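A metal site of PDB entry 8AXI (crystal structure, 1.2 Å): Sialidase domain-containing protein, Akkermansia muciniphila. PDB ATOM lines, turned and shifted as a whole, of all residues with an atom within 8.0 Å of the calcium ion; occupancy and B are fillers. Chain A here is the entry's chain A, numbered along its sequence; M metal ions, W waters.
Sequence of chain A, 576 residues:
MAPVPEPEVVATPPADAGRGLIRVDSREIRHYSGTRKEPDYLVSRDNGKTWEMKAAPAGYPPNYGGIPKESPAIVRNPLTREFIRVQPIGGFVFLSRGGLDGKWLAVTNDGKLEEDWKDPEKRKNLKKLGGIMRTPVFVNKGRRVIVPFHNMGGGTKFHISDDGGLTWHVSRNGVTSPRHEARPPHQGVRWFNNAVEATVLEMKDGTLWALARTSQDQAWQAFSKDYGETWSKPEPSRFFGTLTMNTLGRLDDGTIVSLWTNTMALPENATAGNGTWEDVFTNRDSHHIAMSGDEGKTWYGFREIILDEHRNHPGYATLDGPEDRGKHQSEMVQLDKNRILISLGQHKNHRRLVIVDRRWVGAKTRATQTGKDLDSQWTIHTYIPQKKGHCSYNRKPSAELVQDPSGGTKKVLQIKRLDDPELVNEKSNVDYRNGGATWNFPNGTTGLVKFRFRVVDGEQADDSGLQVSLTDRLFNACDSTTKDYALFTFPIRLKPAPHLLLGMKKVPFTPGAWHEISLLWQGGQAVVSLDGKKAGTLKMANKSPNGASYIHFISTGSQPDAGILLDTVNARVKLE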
ATOM      1  N   HIS A 180      -1.247  22.065 -12.885  1.00  0.00           N
ATOM      2  CA  HIS A 180       0.069  22.678 -12.860  1.00  0.00           C
ATOM      3  C   HIS A 180      -0.038  24.168 -12.567  1.00  0.00           C
ATOM      4  O   HIS A 180      -0.901  24.862 -13.099  1.00  0.00           O
ATOM      5  CB  HIS A 180       0.747  22.484 -14.207  1.00  0.00           C
ATOM      6  CG  HIS A 180       2.081  23.139 -14.305  1.00  0.00           C
ATOM      7  ND1 HIS A 180       2.344  24.144 -15.204  1.00  0.00           N
ATOM      8  CD2 HIS A 180       3.231  22.939 -13.613  1.00  0.00           C
ATOM      9  CE1 HIS A 180       3.597  24.536 -15.069  1.00  0.00           C
ATOM     10  NE2 HIS A 180       4.157  23.834 -14.110  1.00  0.00           N
ATOM     11  N   HIS A 186       8.763  28.169 -15.648  1.00  0.00           N
ATOM     12  CA  HIS A 186       7.670  28.167 -16.614  1.00  0.00           C
ATOM     13  C   HIS A 186       7.202  29.586 -16.916  1.00  0.00           C
ATOM     14  O   HIS A 186       7.177  30.442 -16.032  1.00  0.00           O
ATOM     15  CB  HIS A 186       6.511  27.364 -16.058  1.00  0.00           C
ATOM     16  CG  HIS A 186       6.866  25.949 -15.769  1.00  0.00           C
ATOM     17  ND1 HIS A 186       7.078  25.035 -16.778  1.00  0.00           N
ATOM     18  CD2 HIS A 186       7.050  25.289 -14.607  1.00  0.00           C
ATOM     19  CE1 HIS A 186       7.356  23.857 -16.244  1.00  0.00           C
ATOM     20  NE2 HIS A 186       7.356  23.988 -14.931  1.00  0.00           N
ATOM     21  N   GLY A 188       4.154  29.630 -18.573  1.00  0.00           N
ATOM     22  CA  GLY A 188       2.791  29.263 -18.889  1.00  0.00           C
ATOM     23  C   GLY A 188       2.481  27.963 -18.163  1.00  0.00           C
ATOM     24  O   GLY A 188       3.311  27.442 -17.408  1.00  0.00           O
ATOM     25  N   VAL A 189       1.277  27.449 -18.393  1.00  0.00           N
ATOM     26  CA  VAL A 189       0.800  26.270 -17.657  1.00  0.00           C
ATOM     27  C   VAL A 189       0.897  25.041 -18.537  1.00  0.00           C
ATOM     28  O   VAL A 189       0.669  25.098 -19.753  1.00  0.00           O
ATOM     29  CB  VAL A 189      -0.638  26.460 -17.129  1.00  0.00           C
ATOM     30  CG1 VAL A 189      -0.702  27.582 -16.102  1.00  0.00           C
ATOM     31  CG2 VAL A 189      -1.603  26.711 -18.274  1.00  0.00           C
ATOM     32  N   ARG A 190       1.222  23.923 -17.915  1.00  0.00           N
ATOM     33  CA  ARG A 190       1.183  22.644 -18.588  1.00  0.00           C
ATOM     34  C   ARG A 190      -0.254  22.231 -18.885  1.00  0.00           C
ATOM     35  O   ARG A 190      -1.192  22.568 -18.152  1.00  0.00           O
ATOM     36  CB  ARG A 190       1.807  21.574 -17.705  1.00  0.00           C
ATOM     37  CG  ARG A 190       3.298  21.744 -17.526  1.00  0.00           C
ATOM     38  CD  ARG A 190       3.849  20.563 -16.732  1.00  0.00           C
ATOM     39  NE  ARG A 190       5.302  20.623 -16.543  1.00  0.00           N
ATOM     40  CZ  ARG A 190       5.936  20.139 -15.486  1.00  0.00           C
ATOM     41  NH1 ARG A 190       5.277  19.600 -14.463  1.00  0.00           N
ATOM     42  NH2 ARG A 190       7.273  20.219 -15.431  1.00  0.00           N
ATOM     43  N   TRP A 191      -0.426  21.463 -19.955  1.00  0.00           N
ATOM     44  CA  TRP A 191      -1.678  20.782 -20.224  1.00  0.00           C
ATOM     45  C   TRP A 191      -2.136  20.054 -18.971  1.00  0.00           C
ATOM     46  O   TRP A 191      -1.376  19.288 -18.389  1.00  0.00           O
ATOM     47  CB  TRP A 191      -1.384  19.737 -21.306  1.00  0.00           C
ATOM     48  CG  TRP A 191      -2.563  18.919 -21.806  1.00  0.00           C
ATOM     49  CD1 TRP A 191      -3.886  19.263 -21.785  1.00  0.00           C
ATOM     50  CD2 TRP A 191      -2.475  17.639 -22.448  1.00  0.00           C
ATOM     51  NE1 TRP A 191      -4.625  18.247 -22.354  1.00  0.00           N
ATOM     52  CE2 TRP A 191      -3.793  17.251 -22.785  1.00  0.00           C
ATOM     53  CE3 TRP A 191      -1.415  16.804 -22.798  1.00  0.00           C
ATOM     54  CZ2 TRP A 191      -4.069  16.055 -23.434  1.00  0.00           C
ATOM     55  CZ3 TRP A 191      -1.695  15.599 -23.425  1.00  0.00           C
ATOM     56  CH2 TRP A 191      -3.015  15.238 -23.747  1.00  0.00           C
ATOM     57  N   PHE A 192      -3.384  20.308 -18.557  1.00  0.00           N
ATOM     58  CA  PHE A 192      -3.973  19.641 -17.396  1.00  0.00           C
ATOM     59  C   PHE A 192      -4.489  18.257 -17.738  1.00  0.00           C
ATOM     60  O   PHE A 192      -5.368  18.102 -18.592  1.00  0.00           O
ATOM     61  CB  PHE A 192      -5.112  20.479 -16.827  1.00  0.00           C
ATOM     62  CG  PHE A 192      -5.747  19.858 -15.613  1.00  0.00           C
ATOM     63  CD1 PHE A 192      -4.953  19.345 -14.587  1.00  0.00           C
ATOM     64  CD2 PHE A 192      -7.128  19.811 -15.469  1.00  0.00           C
ATOM     65  CE1 PHE A 192      -5.529  18.752 -13.452  1.00  0.00           C
ATOM     66  CE2 PHE A 192      -7.709  19.234 -14.338  1.00  0.00           C
ATOM     67  CZ  PHE A 192      -6.895  18.726 -13.324  1.00  0.00           C
ATOM     68  N   LEU A 243       2.696  13.784 -18.006  1.00  0.00           N
ATOM     69  CA  LEU A 243       1.847  13.690 -19.202  1.00  0.00           C
ATOM     70  C   LEU A 243       2.295  12.527 -20.083  1.00  0.00           C
ATOM     71  O   LEU A 243       2.241  12.601 -21.313  1.00  0.00           O
ATOM     72  CB  LEU A 243       1.745  15.023 -19.976  1.00  0.00           C
ATOM     73  CG  LEU A 243       1.121  16.178 -19.150  1.00  0.00           C
ATOM     74  CD1 LEU A 243       1.431  17.519 -19.800  1.00  0.00           C
ATOM     75  CD2 LEU A 243      -0.405  15.983 -18.982  1.00  0.00           C
ATOM     76  N   ALA A 265      10.034  17.540 -18.951  1.00  0.00           N
ATOM     77  CA  ALA A 265       9.798  18.379 -20.122  1.00  0.00           C
ATOM     78  C   ALA A 265      10.527  19.716 -19.979  1.00  0.00           C
ATOM     79  O   ALA A 265      10.916  20.122 -18.878  1.00  0.00           O
ATOM     80  CB  ALA A 265       8.307  18.676 -20.259  1.00  0.00           C
ATOM     81  N   LEU A 266      10.732  20.393 -21.109  1.00  0.00           N
ATOM     82  CA  LEU A 266      11.215  21.758 -21.067  1.00  0.00           C
ATOM     83  C   LEU A 266      10.193  22.637 -20.338  1.00  0.00           C
ATOM     84  O   LEU A 266       8.983  22.404 -20.429  1.00  0.00           O
ATOM     85  CB  LEU A 266      11.402  22.303 -22.495  1.00  0.00           C
ATOM     86  CG  LEU A 266      12.713  21.894 -23.155  1.00  0.00           C
ATOM     87  CD1 LEU A 266      12.710  22.274 -24.630  1.00  0.00           C
ATOM     88  CD2 LEU A 266      13.932  22.470 -22.427  1.00  0.00           C
ATOM     89  N   PRO A 267      10.658  23.664 -19.642  1.00  0.00           N
ATOM     90  CA  PRO A 267       9.736  24.653 -19.076  1.00  0.00           C
ATOM     91  C   PRO A 267       8.747  25.149 -20.110  1.00  0.00           C
ATOM     92  O   PRO A 267       9.072  25.313 -21.297  1.00  0.00           O
ATOM     93  CB  PRO A 267      10.655  25.785 -18.617  1.00  0.00           C
ATOM     94  CG  PRO A 267      11.961  25.124 -18.414  1.00  0.00           C
ATOM     95  CD  PRO A 267      12.070  24.094 -19.488  1.00  0.00           C
ATOM     96  N   GLU A 268       7.541  25.432 -19.651  1.00  0.00           N
ATOM     97  CA  GLU A 268       6.528  25.991 -20.524  1.00  0.00           C
ATOM     98  C   GLU A 268       6.960  27.362 -21.045  1.00  0.00           C
ATOM     99  O   GLU A 268       7.579  28.151 -20.334  1.00  0.00           O
ATOM    100  CB  GLU A 268       5.243  26.135 -19.721  1.00  0.00           C
ATOM    101  CG  GLU A 268       4.374  24.902 -19.448  1.00  0.00           C
ATOM    102  CD  GLU A 268       4.284  23.964 -20.626  1.00  0.00           C
ATOM    103  OE1 GLU A 268       3.762  24.424 -21.679  1.00  0.00           O
ATOM    104  OE2 GLU A 268       4.435  22.719 -20.478  1.00  0.00           O
ATOM    105  N   ASN A 269       6.605  27.668 -22.293  1.00  0.00           N
ATOM    106  CA  ASN A 269       6.947  28.935 -22.931  1.00  0.00           C
ATOM    107  C   ASN A 269       5.808  29.928 -22.824  1.00  0.00           C
ATOM    108  O   ASN A 269       4.789  29.685 -22.152  1.00  0.00           O
ATOM    109  CB  ASN A 269       7.388  28.673 -24.379  1.00  0.00           C
ATOM    110  CG  ASN A 269       6.264  28.160 -25.282  1.00  0.00           C
ATOM    111  OD1 ASN A 269       5.103  28.573 -25.156  1.00  0.00           O
ATOM    112  ND2 ASN A 269       6.624  27.313 -26.262  1.00  0.00           N
ATOM    113  N   THR A 271       3.704  31.054 -24.940  1.00  0.00           N
ATOM    114  CA  THR A 271       2.515  30.796 -25.741  1.00  0.00           C
ATOM    115  C   THR A 271       1.961  29.402 -25.459  1.00  0.00           C
ATOM    116  O   THR A 271       1.466  28.722 -26.368  1.00  0.00           O
ATOM    117  CB  THR A 271       2.810  30.955 -27.226  1.00  0.00           C
ATOM    118  OG1 THR A 271       3.901  30.094 -27.598  1.00  0.00           O
ATOM    119  CG2 THR A 271       3.157  32.390 -27.549  1.00  0.00           C
ATOM    120  N   ALA A 272       2.050  28.933 -24.215  1.00  0.00           N
ATOM    121  CA  ALA A 272       1.736  27.534 -23.888  1.00  0.00           C
ATOM    122  C   ALA A 272       0.245  27.224 -23.941  1.00  0.00           C
ATOM    123  O   ALA A 272      -0.110  26.031 -23.951  1.00  0.00           O
ATOM    124  CB  ALA A 272       2.310  27.146 -22.523  1.00  0.00           C
ATOM    125  N   GLY A 273      -0.628  28.232 -23.974  1.00  0.00           N
ATOM    126  CA  GLY A 273      -2.057  28.003 -23.971  1.00  0.00           C
ATOM    127  C   GLY A 273      -2.626  27.934 -22.571  1.00  0.00           C
ATOM    128  O   GLY A 273      -1.932  28.078 -21.567  1.00  0.00           O
ATOM    129  N   GLY A 275      -3.974  25.365 -21.042  1.00  0.00           N
ATOM    130  CA  GLY A 275      -3.901  24.083 -20.389  1.00  0.00           C
ATOM    131  C   GLY A 275      -5.020  23.116 -20.690  1.00  0.00           C
ATOM    132  O   GLY A 275      -4.962  21.978 -20.215  1.00  0.00           O
ATOM    133  N   TRP A 277      -5.523  21.795 -23.700  1.00  0.00           N
ATOM    134  CA  TRP A 277      -4.794  20.859 -24.534  1.00  0.00           C
ATOM    135  C   TRP A 277      -3.309  21.212 -24.509  1.00  0.00           C
ATOM    136  O   TRP A 277      -2.896  22.221 -23.931  1.00  0.00           O
ATOM    137  CB  TRP A 277      -5.339  20.831 -25.980  1.00  0.00           C
ATOM    138  CG  TRP A 277      -6.760  20.290 -26.114  1.00  0.00           C
ATOM    139  CD1 TRP A 277      -7.885  21.020 -26.395  1.00  0.00           C
ATOM    140  CD2 TRP A 277      -7.185  18.924 -26.019  1.00  0.00           C
ATOM    141  NE1 TRP A 277      -8.985  20.185 -26.456  1.00  0.00           N
ATOM    142  CE2 TRP A 277      -8.583  18.900 -26.239  1.00  0.00           C
ATOM    143  CE3 TRP A 277      -6.520  17.719 -25.774  1.00  0.00           C
ATOM    144  CZ2 TRP A 277      -9.329  17.716 -26.190  1.00  0.00           C
ATOM    145  CZ3 TRP A 277      -7.261  16.542 -25.731  1.00  0.00           C
ATOM    146  CH2 TRP A 277      -8.647  16.552 -25.952  1.00  0.00           C
ATOM    147  N   GLU A 278      -2.513  20.332 -25.098  1.00  0.00           N
ATOM    148  CA  GLU A 278      -1.068  20.519 -25.142  1.00  0.00           C
ATOM    149  C   GLU A 278      -0.659  21.517 -26.216  1.00  0.00           C
ATOM    150  O   GLU A 278      -1.348  21.694 -27.233  1.00  0.00           O
ATOM    151  CB  GLU A 278      -0.439  19.164 -25.460  1.00  0.00           C
ATOM    152  CG  GLU A 278       1.081  19.165 -25.421  1.00  0.00           C
ATOM    153  CD  GLU A 278       1.613  19.685 -24.092  1.00  0.00           C
ATOM    154  OE1 GLU A 278       1.708  18.881 -23.122  1.00  0.00           O
ATOM    155  OE2 GLU A 278       1.947  20.896 -24.020  1.00  0.00           O
ATOM    156  N   ASP A 279       0.443  22.245 -25.959  1.00  0.00           N
ATOM    157  CA  ASP A 279       1.051  23.028 -27.039  1.00  0.00           C
ATOM    158  C   ASP A 279       2.111  22.239 -27.786  1.00  0.00           C
ATOM    159  O   ASP A 279       2.117  22.200 -29.028  1.00  0.00           O
ATOM    160  CB  ASP A 279       1.539  24.423 -26.573  1.00  0.00           C
ATOM    161  CG  ASP A 279       2.744  24.383 -25.627  1.00  0.00           C
ATOM    162  OD1 ASP A 279       2.790  23.545 -24.713  1.00  0.00           O
ATOM    163  OD2 ASP A 279       3.609  25.282 -25.742  1.00  0.00           O
ATOM    164  N   VAL A 280       3.031  21.610 -27.066  1.00  0.00           N
ATOM    165  CA  VAL A 280       4.124  20.893 -27.698  1.00  0.00           C
ATOM    166  C   VAL A 280       4.671  19.848 -26.722  1.00  0.00           C
ATOM    167  O   VAL A 280       4.781  20.102 -25.524  1.00  0.00           O
ATOM    168  CB  VAL A 280       5.233  21.863 -28.178  1.00  0.00           C
ATOM    169  CG1 VAL A 280       5.900  22.592 -26.981  1.00  0.00           C
ATOM    170  CG2 VAL A 280       6.244  21.111 -29.023  1.00  0.00           C
ATOM    171  N   PHE A 281       5.015  18.689 -27.249  1.00  0.00           N
ATOM    172  CA  PHE A 281       5.623  17.627 -26.453  1.00  0.00           C
ATOM    173  C   PHE A 281       7.148  17.709 -26.537  1.00  0.00           C
ATOM    174  O   PHE A 281       7.725  17.648 -27.629  1.00  0.00           O
ATOM    175  CB  PHE A 281       5.168  16.271 -26.990  1.00  0.00           C
ATOM    176  CG  PHE A 281       3.716  15.984 -26.733  1.00  0.00           C
ATOM    177  CD1 PHE A 281       3.254  15.891 -25.432  1.00  0.00           C
ATOM    178  CD2 PHE A 281       2.828  15.864 -27.785  1.00  0.00           C
ATOM    179  CE1 PHE A 281       1.908  15.619 -25.181  1.00  0.00           C
ATOM    180  CE2 PHE A 281       1.475  15.594 -27.540  1.00  0.00           C
ATOM    181  CZ  PHE A 281       1.037  15.494 -26.223  1.00  0.00           C
ATOM    182  N   THR A 282       7.798  17.821 -25.385  1.00  0.00           N
ATOM    183  CA  THR A 282       9.252  17.884 -25.330  1.00  0.00           C
ATOM    184  C   THR A 282       9.837  16.819 -24.422  1.00  0.00           C
ATOM    185  O   THR A 282      10.936  16.981 -23.906  1.00  0.00           O
ATOM    186  CB  THR A 282       9.762  19.281 -24.917  1.00  0.00           C
ATOM    187  OG1 THR A 282       9.323  19.565 -23.576  1.00  0.00           O
ATOM    188  CG2 THR A 282       9.251  20.353 -25.878  1.00  0.00           C
HETATM  189 CA    CA M   1       2.947  22.447 -22.625  1.00  0.00          CA
HETATM  190  O   HOH W   1       2.337  20.689 -21.168  1.00  0.00           O
HETATM  191  O   HOH W   2       4.977  21.469 -23.251  1.00  0.00           O
HETATM  192  O   HOH W   3       0.940  23.628 -22.036  1.00  0.00           O
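The backbone NH of Val 280 sits close to the side-chain carboxylate of Glu 278, 3.3 Å away. The backbone NH (N) of Glu 268 is in hydrogen-bond range of a ring nitrogen (ND1) of His 186.
The calcium ion is bound by the side-chain carboxylate (OE2) of Glu 278, water W2, the side-chain carboxylate (OE1) of Glu 268, water W1, the side-chain carboxylate (OD1) of Asp 279, water W3 and the side-chain carboxylate (OE2) of Glu 268. The calcium ion has seven donor atoms within binding distance.
Water W1 bridges the side-chain carboxylate (OE1) of Glu 278 and the backbone NH (N) of Trp 191. Water W3 lies within hydrogen-bond range of the backbone carbonyl oxygen of Val 189 (2.7 Å), the backbone carbonyl oxygen of Ala 272 (3.2 Å) and the backbone NH of Trp 191 (3.3 Å).
Of the 23 residues printed, 3 come within 4 Å of the calcium ion.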
